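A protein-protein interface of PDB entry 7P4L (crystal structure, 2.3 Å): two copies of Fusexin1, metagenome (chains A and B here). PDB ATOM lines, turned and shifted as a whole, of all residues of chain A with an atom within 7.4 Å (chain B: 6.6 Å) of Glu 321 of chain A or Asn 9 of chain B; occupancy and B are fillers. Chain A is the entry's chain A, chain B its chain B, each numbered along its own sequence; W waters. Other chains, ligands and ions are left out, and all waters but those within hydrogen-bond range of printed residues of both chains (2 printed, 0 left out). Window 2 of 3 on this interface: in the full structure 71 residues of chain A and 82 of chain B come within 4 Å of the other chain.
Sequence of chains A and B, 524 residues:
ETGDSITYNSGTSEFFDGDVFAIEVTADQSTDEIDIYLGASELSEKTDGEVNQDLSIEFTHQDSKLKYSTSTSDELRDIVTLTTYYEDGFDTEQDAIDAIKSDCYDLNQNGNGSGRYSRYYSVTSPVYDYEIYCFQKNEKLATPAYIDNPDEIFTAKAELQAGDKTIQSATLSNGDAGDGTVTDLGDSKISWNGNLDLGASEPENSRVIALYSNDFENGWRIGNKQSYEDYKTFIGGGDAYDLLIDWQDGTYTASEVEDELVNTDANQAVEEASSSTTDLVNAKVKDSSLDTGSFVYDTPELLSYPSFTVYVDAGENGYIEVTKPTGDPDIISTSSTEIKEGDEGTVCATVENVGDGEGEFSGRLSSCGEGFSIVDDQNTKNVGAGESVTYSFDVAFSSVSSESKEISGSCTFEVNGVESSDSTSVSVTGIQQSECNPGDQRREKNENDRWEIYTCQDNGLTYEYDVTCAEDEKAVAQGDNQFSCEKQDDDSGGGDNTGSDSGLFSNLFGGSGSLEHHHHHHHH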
ATOM      1  N   GLU A  33     -10.549 -27.812   3.281  1.00  0.00           N
ATOM      2  CA  GLU A  33     -11.947 -28.177   3.464  1.00  0.00           C
ATOM      3  C   GLU A  33     -12.706 -27.781   2.207  1.00  0.00           C
ATOM      4  O   GLU A  33     -12.551 -26.659   1.714  1.00  0.00           O
ATOM      5  CB  GLU A  33     -12.550 -27.496   4.699  1.00  0.00           C
ATOM      6  CG  GLU A  33     -11.844 -27.822   6.009  1.00  0.00           C
ATOM      7  CD  GLU A  33     -12.447 -27.085   7.197  1.00  0.00           C
ATOM      8  OE1 GLU A  33     -13.419 -26.327   6.998  1.00  0.00           O
ATOM      9  OE2 GLU A  33     -11.948 -27.260   8.330  1.00  0.00           O
ATOM     10  N   ILE A  34     -13.501 -28.706   1.677  1.00  0.00           N
ATOM     11  CA  ILE A  34     -14.283 -28.466   0.468  1.00  0.00           C
ATOM     12  C   ILE A  34     -15.634 -27.913   0.912  1.00  0.00           C
ATOM     13  O   ILE A  34     -16.489 -28.650   1.399  1.00  0.00           O
ATOM     14  CB  ILE A  34     -14.437 -29.737  -0.369  1.00  0.00           C
ATOM     15  CG1 ILE A  34     -13.067 -30.311  -0.745  1.00  0.00           C
ATOM     16  CG2 ILE A  34     -15.247 -29.447  -1.620  1.00  0.00           C
ATOM     17  CD1 ILE A  34     -12.247 -29.418  -1.665  1.00  0.00           C
ATOM     18  N   ASP A  35     -15.830 -26.609   0.737  1.00  0.00           N
ATOM     19  CA  ASP A  35     -17.063 -25.945   1.148  1.00  0.00           C
ATOM     20  C   ASP A  35     -18.075 -25.987   0.008  1.00  0.00           C
ATOM     21  O   ASP A  35     -17.785 -25.532  -1.104  1.00  0.00           O
ATOM     22  CB  ASP A  35     -16.787 -24.503   1.569  1.00  0.00           C
ATOM     23  CG  ASP A  35     -15.831 -24.414   2.741  1.00  0.00           C
ATOM     24  OD1 ASP A  35     -15.879 -25.297   3.627  1.00  0.00           O
ATOM     25  OD2 ASP A  35     -15.025 -23.463   2.773  1.00  0.00           O
ATOM     26  N   ILE A  36     -19.261 -26.524   0.292  1.00  0.00           N
ATOM     27  CA  ILE A  36     -20.308 -26.724  -0.703  1.00  0.00           C
ATOM     28  C   ILE A  36     -21.382 -25.662  -0.518  1.00  0.00           C
ATOM     29  O   ILE A  36     -21.871 -25.445   0.598  1.00  0.00           O
ATOM     30  CB  ILE A  36     -20.920 -28.130  -0.597  1.00  0.00           C
ATOM     31  CG1 ILE A  36     -19.841 -29.203  -0.763  1.00  0.00           C
ATOM     32  CG2 ILE A  36     -22.012 -28.301  -1.645  1.00  0.00           C
ATOM     33  CD1 ILE A  36     -20.297 -30.602  -0.381  1.00  0.00           C
ATOM     34  N   TYR A  37     -21.749 -25.003  -1.613  1.00  0.00           N
ATOM     35  CA  TYR A  37     -22.807 -24.003  -1.621  1.00  0.00           C
ATOM     36  C   TYR A  37     -23.869 -24.435  -2.620  1.00  0.00           C
ATOM     37  O   TYR A  37     -23.544 -24.801  -3.754  1.00  0.00           O
ATOM     38  CB  TYR A  37     -22.258 -22.621  -1.984  1.00  0.00           C
ATOM     39  CG  TYR A  37     -21.350 -22.032  -0.926  1.00  0.00           C
ATOM     40  CD1 TYR A  37     -21.867 -21.314   0.144  1.00  0.00           C
ATOM     41  CD2 TYR A  37     -19.973 -22.196  -0.998  1.00  0.00           C
ATOM     42  CE1 TYR A  37     -21.036 -20.772   1.111  1.00  0.00           C
ATOM     43  CE2 TYR A  37     -19.138 -21.659  -0.040  1.00  0.00           C
ATOM     44  CZ  TYR A  37     -19.671 -20.952   1.012  1.00  0.00           C
ATOM     45  OH  TYR A  37     -18.835 -20.421   1.967  1.00  0.00           O
ATOM     46  N   LEU A  55     -22.138 -26.824   3.578  1.00  0.00           N
ATOM     47  CA  LEU A  55     -21.660 -28.148   3.934  1.00  0.00           C
ATOM     48  C   LEU A  55     -20.190 -28.213   3.562  1.00  0.00           C
ATOM     49  O   LEU A  55     -19.777 -27.640   2.548  1.00  0.00           O
ATOM     50  CB  LEU A  55     -22.434 -29.255   3.208  1.00  0.00           C
ATOM     51  CG  LEU A  55     -23.831 -29.618   3.702  1.00  0.00           C
ATOM     52  CD1 LEU A  55     -24.560 -30.407   2.632  1.00  0.00           C
ATOM     53  CD2 LEU A  55     -23.750 -30.421   4.989  1.00  0.00           C
ATOM     54  N   SER A  56     -19.398 -28.897   4.376  1.00  0.00           N
ATOM     55  CA  SER A  56     -17.978 -29.014   4.089  1.00  0.00           C
ATOM     56  C   SER A  56     -17.527 -30.463   4.213  1.00  0.00           C
ATOM     57  O   SER A  56     -17.987 -31.200   5.090  1.00  0.00           O
ATOM     58  CB  SER A  56     -17.148 -28.114   5.019  1.00  0.00           C
ATOM     59  OG  SER A  56     -17.222 -28.552   6.364  1.00  0.00           O
ATOM     60  N   ILE A  57     -16.649 -30.864   3.295  1.00  0.00           N
ATOM     61  CA  ILE A  57     -16.032 -32.185   3.269  1.00  0.00           C
ATOM     62  C   ILE A  57     -14.536 -32.022   3.494  1.00  0.00           C
ATOM     63  O   ILE A  57     -13.916 -31.104   2.947  1.00  0.00           O
ATOM     64  CB  ILE A  57     -16.296 -32.915   1.936  1.00  0.00           C
ATOM     65  CG1 ILE A  57     -17.792 -33.175   1.762  1.00  0.00           C
ATOM     66  CG2 ILE A  57     -15.539 -34.220   1.897  1.00  0.00           C
ATOM     67  CD1 ILE A  57     -18.165 -33.730   0.414  1.00  0.00           C
ATOM     68  N   TYR A 319     -21.739 -24.443  -6.519  1.00  0.00           N
ATOM     69  CA  TYR A 319     -20.301 -24.250  -6.640  1.00  0.00           C
ATOM     70  C   TYR A 319     -19.580 -24.680  -5.369  1.00  0.00           C
ATOM     71  O   TYR A 319     -20.191 -25.043  -4.359  1.00  0.00           O
ATOM     72  CB  TYR A 319     -19.959 -22.792  -6.964  1.00  0.00           C
ATOM     73  CG  TYR A 319     -20.374 -21.799  -5.905  1.00  0.00           C
ATOM     74  CD1 TYR A 319     -21.661 -21.278  -5.876  1.00  0.00           C
ATOM     75  CD2 TYR A 319     -19.476 -21.383  -4.934  1.00  0.00           C
ATOM     76  CE1 TYR A 319     -22.040 -20.364  -4.911  1.00  0.00           C
ATOM     77  CE2 TYR A 319     -19.845 -20.474  -3.962  1.00  0.00           C
ATOM     78  CZ  TYR A 319     -21.127 -19.968  -3.954  1.00  0.00           C
ATOM     79  OH  TYR A 319     -21.487 -19.063  -2.981  1.00  0.00           O
ATOM     80  N   ILE A 320     -18.251 -24.638  -5.450  1.00  0.00           N
ATOM     81  CA  ILE A 320     -17.362 -25.078  -4.386  1.00  0.00           C
ATOM     82  C   ILE A 320     -16.386 -23.961  -4.061  1.00  0.00           C
ATOM     83  O   ILE A 320     -16.000 -23.168  -4.926  1.00  0.00           O
ATOM     84  CB  ILE A 320     -16.596 -26.357  -4.790  1.00  0.00           C
ATOM     85  CG1 ILE A 320     -17.570 -27.515  -4.985  1.00  0.00           C
ATOM     86  CG2 ILE A 320     -15.533 -26.709  -3.768  1.00  0.00           C
ATOM     87  CD1 ILE A 320     -18.363 -27.889  -3.755  1.00  0.00           C
ATOM     88  N   GLU A 321     -15.990 -23.903  -2.795  1.00  0.00           N
ATOM     89  CA  GLU A 321     -14.862 -23.096  -2.362  1.00  0.00           C
ATOM     90  C   GLU A 321     -13.984 -23.965  -1.473  1.00  0.00           C
ATOM     91  O   GLU A 321     -14.392 -25.042  -1.030  1.00  0.00           O
ATOM     92  CB  GLU A 321     -15.314 -21.830  -1.625  1.00  0.00           C
ATOM     93  CG  GLU A 321     -16.293 -20.975  -2.435  1.00  0.00           C
ATOM     94  CD  GLU A 321     -16.515 -19.600  -1.837  1.00  0.00           C
ATOM     95  OE1 GLU A 321     -16.043 -19.361  -0.705  1.00  0.00           O
ATOM     96  OE2 GLU A 321     -17.156 -18.754  -2.504  1.00  0.00           O
ATOM     97  N   VAL A 322     -12.762 -23.507  -1.237  1.00  0.00           N
ATOM     98  CA  VAL A 322     -11.812 -24.213  -0.389  1.00  0.00           C
ATOM     99  C   VAL A 322     -11.428 -23.300   0.764  1.00  0.00           C
ATOM    100  O   VAL A 322     -11.062 -22.141   0.549  1.00  0.00           O
ATOM    101  CB  VAL A 322     -10.564 -24.651  -1.176  1.00  0.00           C
ATOM    102  CG1 VAL A 322      -9.582 -25.353  -0.260  1.00  0.00           C
ATOM    103  CG2 VAL A 322     -10.959 -25.555  -2.318  1.00  0.00           C
ATOM    104  N   THR A 323     -11.517 -23.820   1.982  1.00  0.00           N
ATOM    105  CA  THR A 323     -11.019 -23.134   3.165  1.00  0.00           C
ATOM    106  C   THR A 323      -9.745 -23.833   3.621  1.00  0.00           C
ATOM    107  O   THR A 323      -9.754 -25.042   3.869  1.00  0.00           O
ATOM    108  CB  THR A 323     -12.068 -23.121   4.279  1.00  0.00           C
ATOM    109  OG1 THR A 323     -13.147 -22.249   3.912  1.00  0.00           O
ATOM    110  CG2 THR A 323     -11.455 -22.654   5.594  1.00  0.00           C
ATOM    111  N   LYS A 324      -8.659 -23.068   3.739  1.00  0.00           N
ATOM    112  CA  LYS A 324      -7.342 -23.598   4.087  1.00  0.00           C
ATOM    113  C   LYS A 324      -6.831 -22.898   5.339  1.00  0.00           C
ATOM    114  O   LYS A 324      -6.203 -21.831   5.254  1.00  0.00           O
ATOM    115  CB  LYS A 324      -6.348 -23.430   2.937  1.00  0.00           C
ATOM    116  CG  LYS A 324      -4.991 -24.085   3.222  1.00  0.00           C
ATOM    117  CD  LYS A 324      -4.003 -23.917   2.076  1.00  0.00           C
ATOM    118  CE  LYS A 324      -4.100 -25.012   1.039  1.00  0.00           C
ATOM    119  NZ  LYS A 324      -3.405 -26.245   1.495  1.00  0.00           N
ATOM    120  N   PRO A 325      -7.073 -23.459   6.520  1.00  0.00           N
ATOM    121  CA  PRO A 325      -6.417 -22.942   7.724  1.00  0.00           C
ATOM    122  C   PRO A 325      -4.911 -23.149   7.652  1.00  0.00           C
ATOM    123  O   PRO A 325      -4.416 -24.064   6.988  1.00  0.00           O
ATOM    124  CB  PRO A 325      -7.038 -23.769   8.857  1.00  0.00           C
ATOM    125  CG  PRO A 325      -8.301 -24.320   8.293  1.00  0.00           C
ATOM    126  CD  PRO A 325      -8.059 -24.508   6.833  1.00  0.00           C
ATOM    127  N   ILE B   6     -10.585 -20.962  -8.624  1.00  0.00           N
ATOM    128  CA  ILE B   6     -11.201 -21.568  -7.449  1.00  0.00           C
ATOM    129  C   ILE B   6     -11.036 -20.603  -6.286  1.00  0.00           C
ATOM    130  O   ILE B   6      -9.919 -20.157  -6.000  1.00  0.00           O
ATOM    131  CB  ILE B   6     -10.575 -22.934  -7.111  1.00  0.00           C
ATOM    132  CG1 ILE B   6     -10.787 -23.932  -8.257  1.00  0.00           C
ATOM    133  CG2 ILE B   6     -11.159 -23.477  -5.811  1.00  0.00           C
ATOM    134  CD1 ILE B   6     -12.240 -24.250  -8.554  1.00  0.00           C
ATOM    135  N   THR B   7     -12.139 -20.268  -5.631  1.00  0.00           N
ATOM    136  CA  THR B   7     -12.079 -19.331  -4.523  1.00  0.00           C
ATOM    137  C   THR B   7     -11.504 -20.006  -3.285  1.00  0.00           C
ATOM    138  O   THR B   7     -11.858 -21.142  -2.955  1.00  0.00           O
ATOM    139  CB  THR B   7     -13.467 -18.767  -4.228  1.00  0.00           C
ATOM    140  OG1 THR B   7     -13.905 -17.997  -5.354  1.00  0.00           O
ATOM    141  CG2 THR B   7     -13.446 -17.889  -2.976  1.00  0.00           C
ATOM    142  N   TYR B   8     -10.619 -19.291  -2.595  1.00  0.00           N
ATOM    143  CA  TYR B   8      -9.981 -19.772  -1.379  1.00  0.00           C
ATOM    144  C   TYR B   8     -10.311 -18.844  -0.221  1.00  0.00           C
ATOM    145  O   TYR B   8     -10.407 -17.626  -0.398  1.00  0.00           O
ATOM    146  CB  TYR B   8      -8.459 -19.869  -1.551  1.00  0.00           C
ATOM    147  CG  TYR B   8      -7.996 -21.209  -2.060  1.00  0.00           C
ATOM    148  CD1 TYR B   8      -8.135 -21.549  -3.397  1.00  0.00           C
ATOM    149  CD2 TYR B   8      -7.426 -22.139  -1.203  1.00  0.00           C
ATOM    150  CE1 TYR B   8      -7.723 -22.771  -3.868  1.00  0.00           C
ATOM    151  CE2 TYR B   8      -7.005 -23.369  -1.667  1.00  0.00           C
ATOM    152  CZ  TYR B   8      -7.158 -23.680  -3.001  1.00  0.00           C
ATOM    153  OH  TYR B   8      -6.747 -24.906  -3.470  1.00  0.00           O
ATOM    154  N   ASN B   9     -10.475 -19.428   0.963  1.00  0.00           N
ATOM    155  CA  ASN B   9     -10.780 -18.691   2.176  1.00  0.00           C
ATOM    156  C   ASN B   9      -9.872 -19.183   3.292  1.00  0.00           C
ATOM    157  O   ASN B   9      -9.472 -20.348   3.320  1.00  0.00           O
ATOM    158  CB  ASN B   9     -12.247 -18.853   2.606  1.00  0.00           C
ATOM    159  CG  ASN B   9     -13.223 -18.395   1.542  1.00  0.00           C
ATOM    160  OD1 ASN B   9     -13.097 -17.299   0.998  1.00  0.00           O
ATOM    161  ND2 ASN B   9     -14.222 -19.224   1.260  1.00  0.00           N
ATOM    162  N   SER B  10      -9.544 -18.278   4.208  1.00  0.00           N
ATOM    163  CA  SER B  10      -8.742 -18.635   5.368  1.00  0.00           C
ATOM    164  C   SER B  10      -8.783 -17.528   6.413  1.00  0.00           C
ATOM    165  O   SER B  10      -8.630 -16.349   6.081  1.00  0.00           O
ATOM    166  CB  SER B  10      -7.297 -18.910   4.961  1.00  0.00           C
ATOM    167  OG  SER B  10      -6.483 -19.010   6.114  1.00  0.00           O
ATOM    168  N   GLY B  11      -8.986 -17.898   7.679  1.00  0.00           N
ATOM    169  CA  GLY B  11      -8.955 -16.911   8.739  1.00  0.00           C
ATOM    170  C   GLY B  11      -7.566 -16.536   9.199  1.00  0.00           C
ATOM    171  O   GLY B  11      -7.385 -15.447   9.756  1.00  0.00           O
ATOM    172  N   SER B  13      -4.483 -16.959   7.155  1.00  0.00           N
ATOM    173  CA  SER B  13      -3.525 -16.660   6.097  1.00  0.00           C
ATOM    174  C   SER B  13      -4.125 -15.637   5.145  1.00  0.00           C
ATOM    175  O   SER B  13      -5.206 -15.859   4.592  1.00  0.00           O
ATOM    176  CB  SER B  13      -3.135 -17.930   5.336  1.00  0.00           C
ATOM    177  OG  SER B  13      -2.433 -17.616   4.144  1.00  0.00           O
ATOM    178  N   PHE B  16      -3.984 -17.138   1.329  1.00  0.00           N
ATOM    179  CA  PHE B  16      -5.065 -18.035   0.954  1.00  0.00           C
ATOM    180  C   PHE B  16      -6.452 -17.445   1.192  1.00  0.00           C
ATOM    181  O   PHE B  16      -7.445 -18.146   0.975  1.00  0.00           O
ATOM    182  CB  PHE B  16      -4.935 -19.368   1.700  1.00  0.00           C
ATOM    183  CG  PHE B  16      -3.824 -20.247   1.185  1.00  0.00           C
ATOM    184  CD1 PHE B  16      -3.867 -20.753  -0.102  1.00  0.00           C
ATOM    185  CD2 PHE B  16      -2.755 -20.590   1.994  1.00  0.00           C
ATOM    186  CE1 PHE B  16      -2.854 -21.569  -0.578  1.00  0.00           C
ATOM    187  CE2 PHE B  16      -1.740 -21.408   1.521  1.00  0.00           C
ATOM    188  CZ  PHE B  16      -1.791 -21.897   0.234  1.00  0.00           C
ATOM    189  N   ASP B  17      -6.553 -16.195   1.649  1.00  0.00           N
ATOM    190  CA  ASP B  17      -7.849 -15.544   1.817  1.00  0.00           C
ATOM    191  C   ASP B  17      -8.270 -14.679   0.637  1.00  0.00           C
ATOM    192  O   ASP B  17      -9.431 -14.263   0.584  1.00  0.00           O
ATOM    193  CB  ASP B  17      -7.855 -14.673   3.078  1.00  0.00           C
ATOM    194  CG  ASP B  17      -9.252 -14.375   3.560  1.00  0.00           C
ATOM    195  OD1 ASP B  17      -9.964 -15.327   3.937  1.00  0.00           O
ATOM    196  OD2 ASP B  17      -9.644 -13.188   3.551  1.00  0.00           O
ATOM    197  N   GLY B  18      -7.383 -14.411  -0.311  1.00  0.00           N
ATOM    198  CA  GLY B  18      -7.735 -13.523  -1.398  1.00  0.00           C
ATOM    199  C   GLY B  18      -8.372 -14.272  -2.549  1.00  0.00           C
ATOM    200  O   GLY B  18      -9.291 -15.073  -2.347  1.00  0.00           O
HETATM  201  O   HOH W   1     -16.367 -20.732   2.139  1.00  0.00           O
HETATM  202  O   HOH W   2     -15.012 -20.951  -5.901  1.00  0.00           O
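The side-chain carboxylate (OE1) of Glu 321 of chain A lies within hydrogen-bond range of the side-chain amide nitrogen (ND2) of Asn 9 of chain B.
The backbone carbonyl oxygen (O) of Thr 7 of chain B lies within hydrogen-bond range of the backbone NH (N) of Val 322 of chain A (3.1 Å).
O of Val 322 of chain A is in hydrogen-bond range of N of Asn 9 of chain B (2.8 Å).
The backbone carbonyl oxygen (O) of Asn 9 of chain B lies within hydrogen-bond range of the backbone NH (N) of Lys 324 of chain A, at 2.9 Å.
The backbone carbonyl oxygen of Lys 324 of chain A lies within hydrogen-bond range of the side-chain hydroxyl of Ser 10 of chain B (3.0 Å).
N of Glu 33 of chain A sits at hydrogen-bond distance from O of Thr 323 of chain A (2.9 Å).
The backbone carbonyl oxygen of Glu 321 of chain A lies within hydrogen-bond range of the backbone NH of Asp 35 of chain A, at 2.8 Å.
The backbone NH (N) of Asn 9 of chain B lies within hydrogen-bond range of the backbone carbonyl oxygen (O) of Phe 16 of chain B (3.3 Å).
The side-chain hydroxyl (OG) of Ser 10 of chain B is in hydrogen-bond range of the backbone NH (N) of Ser 13 of chain B (3.0 Å).
The backbone NH (N) of Ser 10 of chain B is in hydrogen-bond range of the side-chain carboxylate (OD1) of Asp 17 of chain B (3.0 Å).
The backbone NH (N) of Phe 16 of chain B is in hydrogen-bond range of the side-chain hydroxyl (OG) of Ser 13 of chain B (3.2 Å).
CA of Glu 321 of chain A touches O of Thr 7 of chain B, 3.6 Å away.
O of Val 322 of chain A touches CA of Tyr 8 of chain B (3.2 Å).
CA of Thr 323 of chain A touches O of Asn 9 of chain B (3.2 Å).
Phe 16 of chain B touches Lys 324 of chain A.
Of the printed residues of chain B, Glu 321 of chain A touches Thr 7 and Asn 9.
Printed residues of chain B within 4 Å of Thr 323 of chain A: Asn 9.
Printed residues of chain A within 4 Å of Tyr 8 of chain B: Val 322 (3.2 Å).
Of chain A, only Glu 321 (2.7 Å), Val 322 (2.8 Å), Thr 323 (3.2 Å) and Lys 324 (2.9 Å) come within 4 Å of Asn 9 of chain B.
Printed residues of chain A within 4 Å of Phe 16 of chain B: Lys 324 (3.4 Å).
The nearest printed residue of chain B that does not touch Lys 324 of chain A is Tyr 8 of chain B (4.3 Å).
Printed residues of chain B that touch a printed residue of chain A: Thr 7, Tyr 8, Asn 9, Ser 10 and Phe 16.
No position is printed for both chains.
Water W1 lies within hydrogen-bond range of OH of Tyr 37 of chain A (2.5 Å), ND2 of Asn 9 of chain B (2.8 Å), OD2 of Asp 35 of chain A (3.1 Å) and OE1 of Glu 321 of chain A (3.2 Å).
Water W2 lies within hydrogen-bond range of O of Ile 320 of chain A (2.6 Å) and N of Thr 7 of chain B (3.0 Å).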
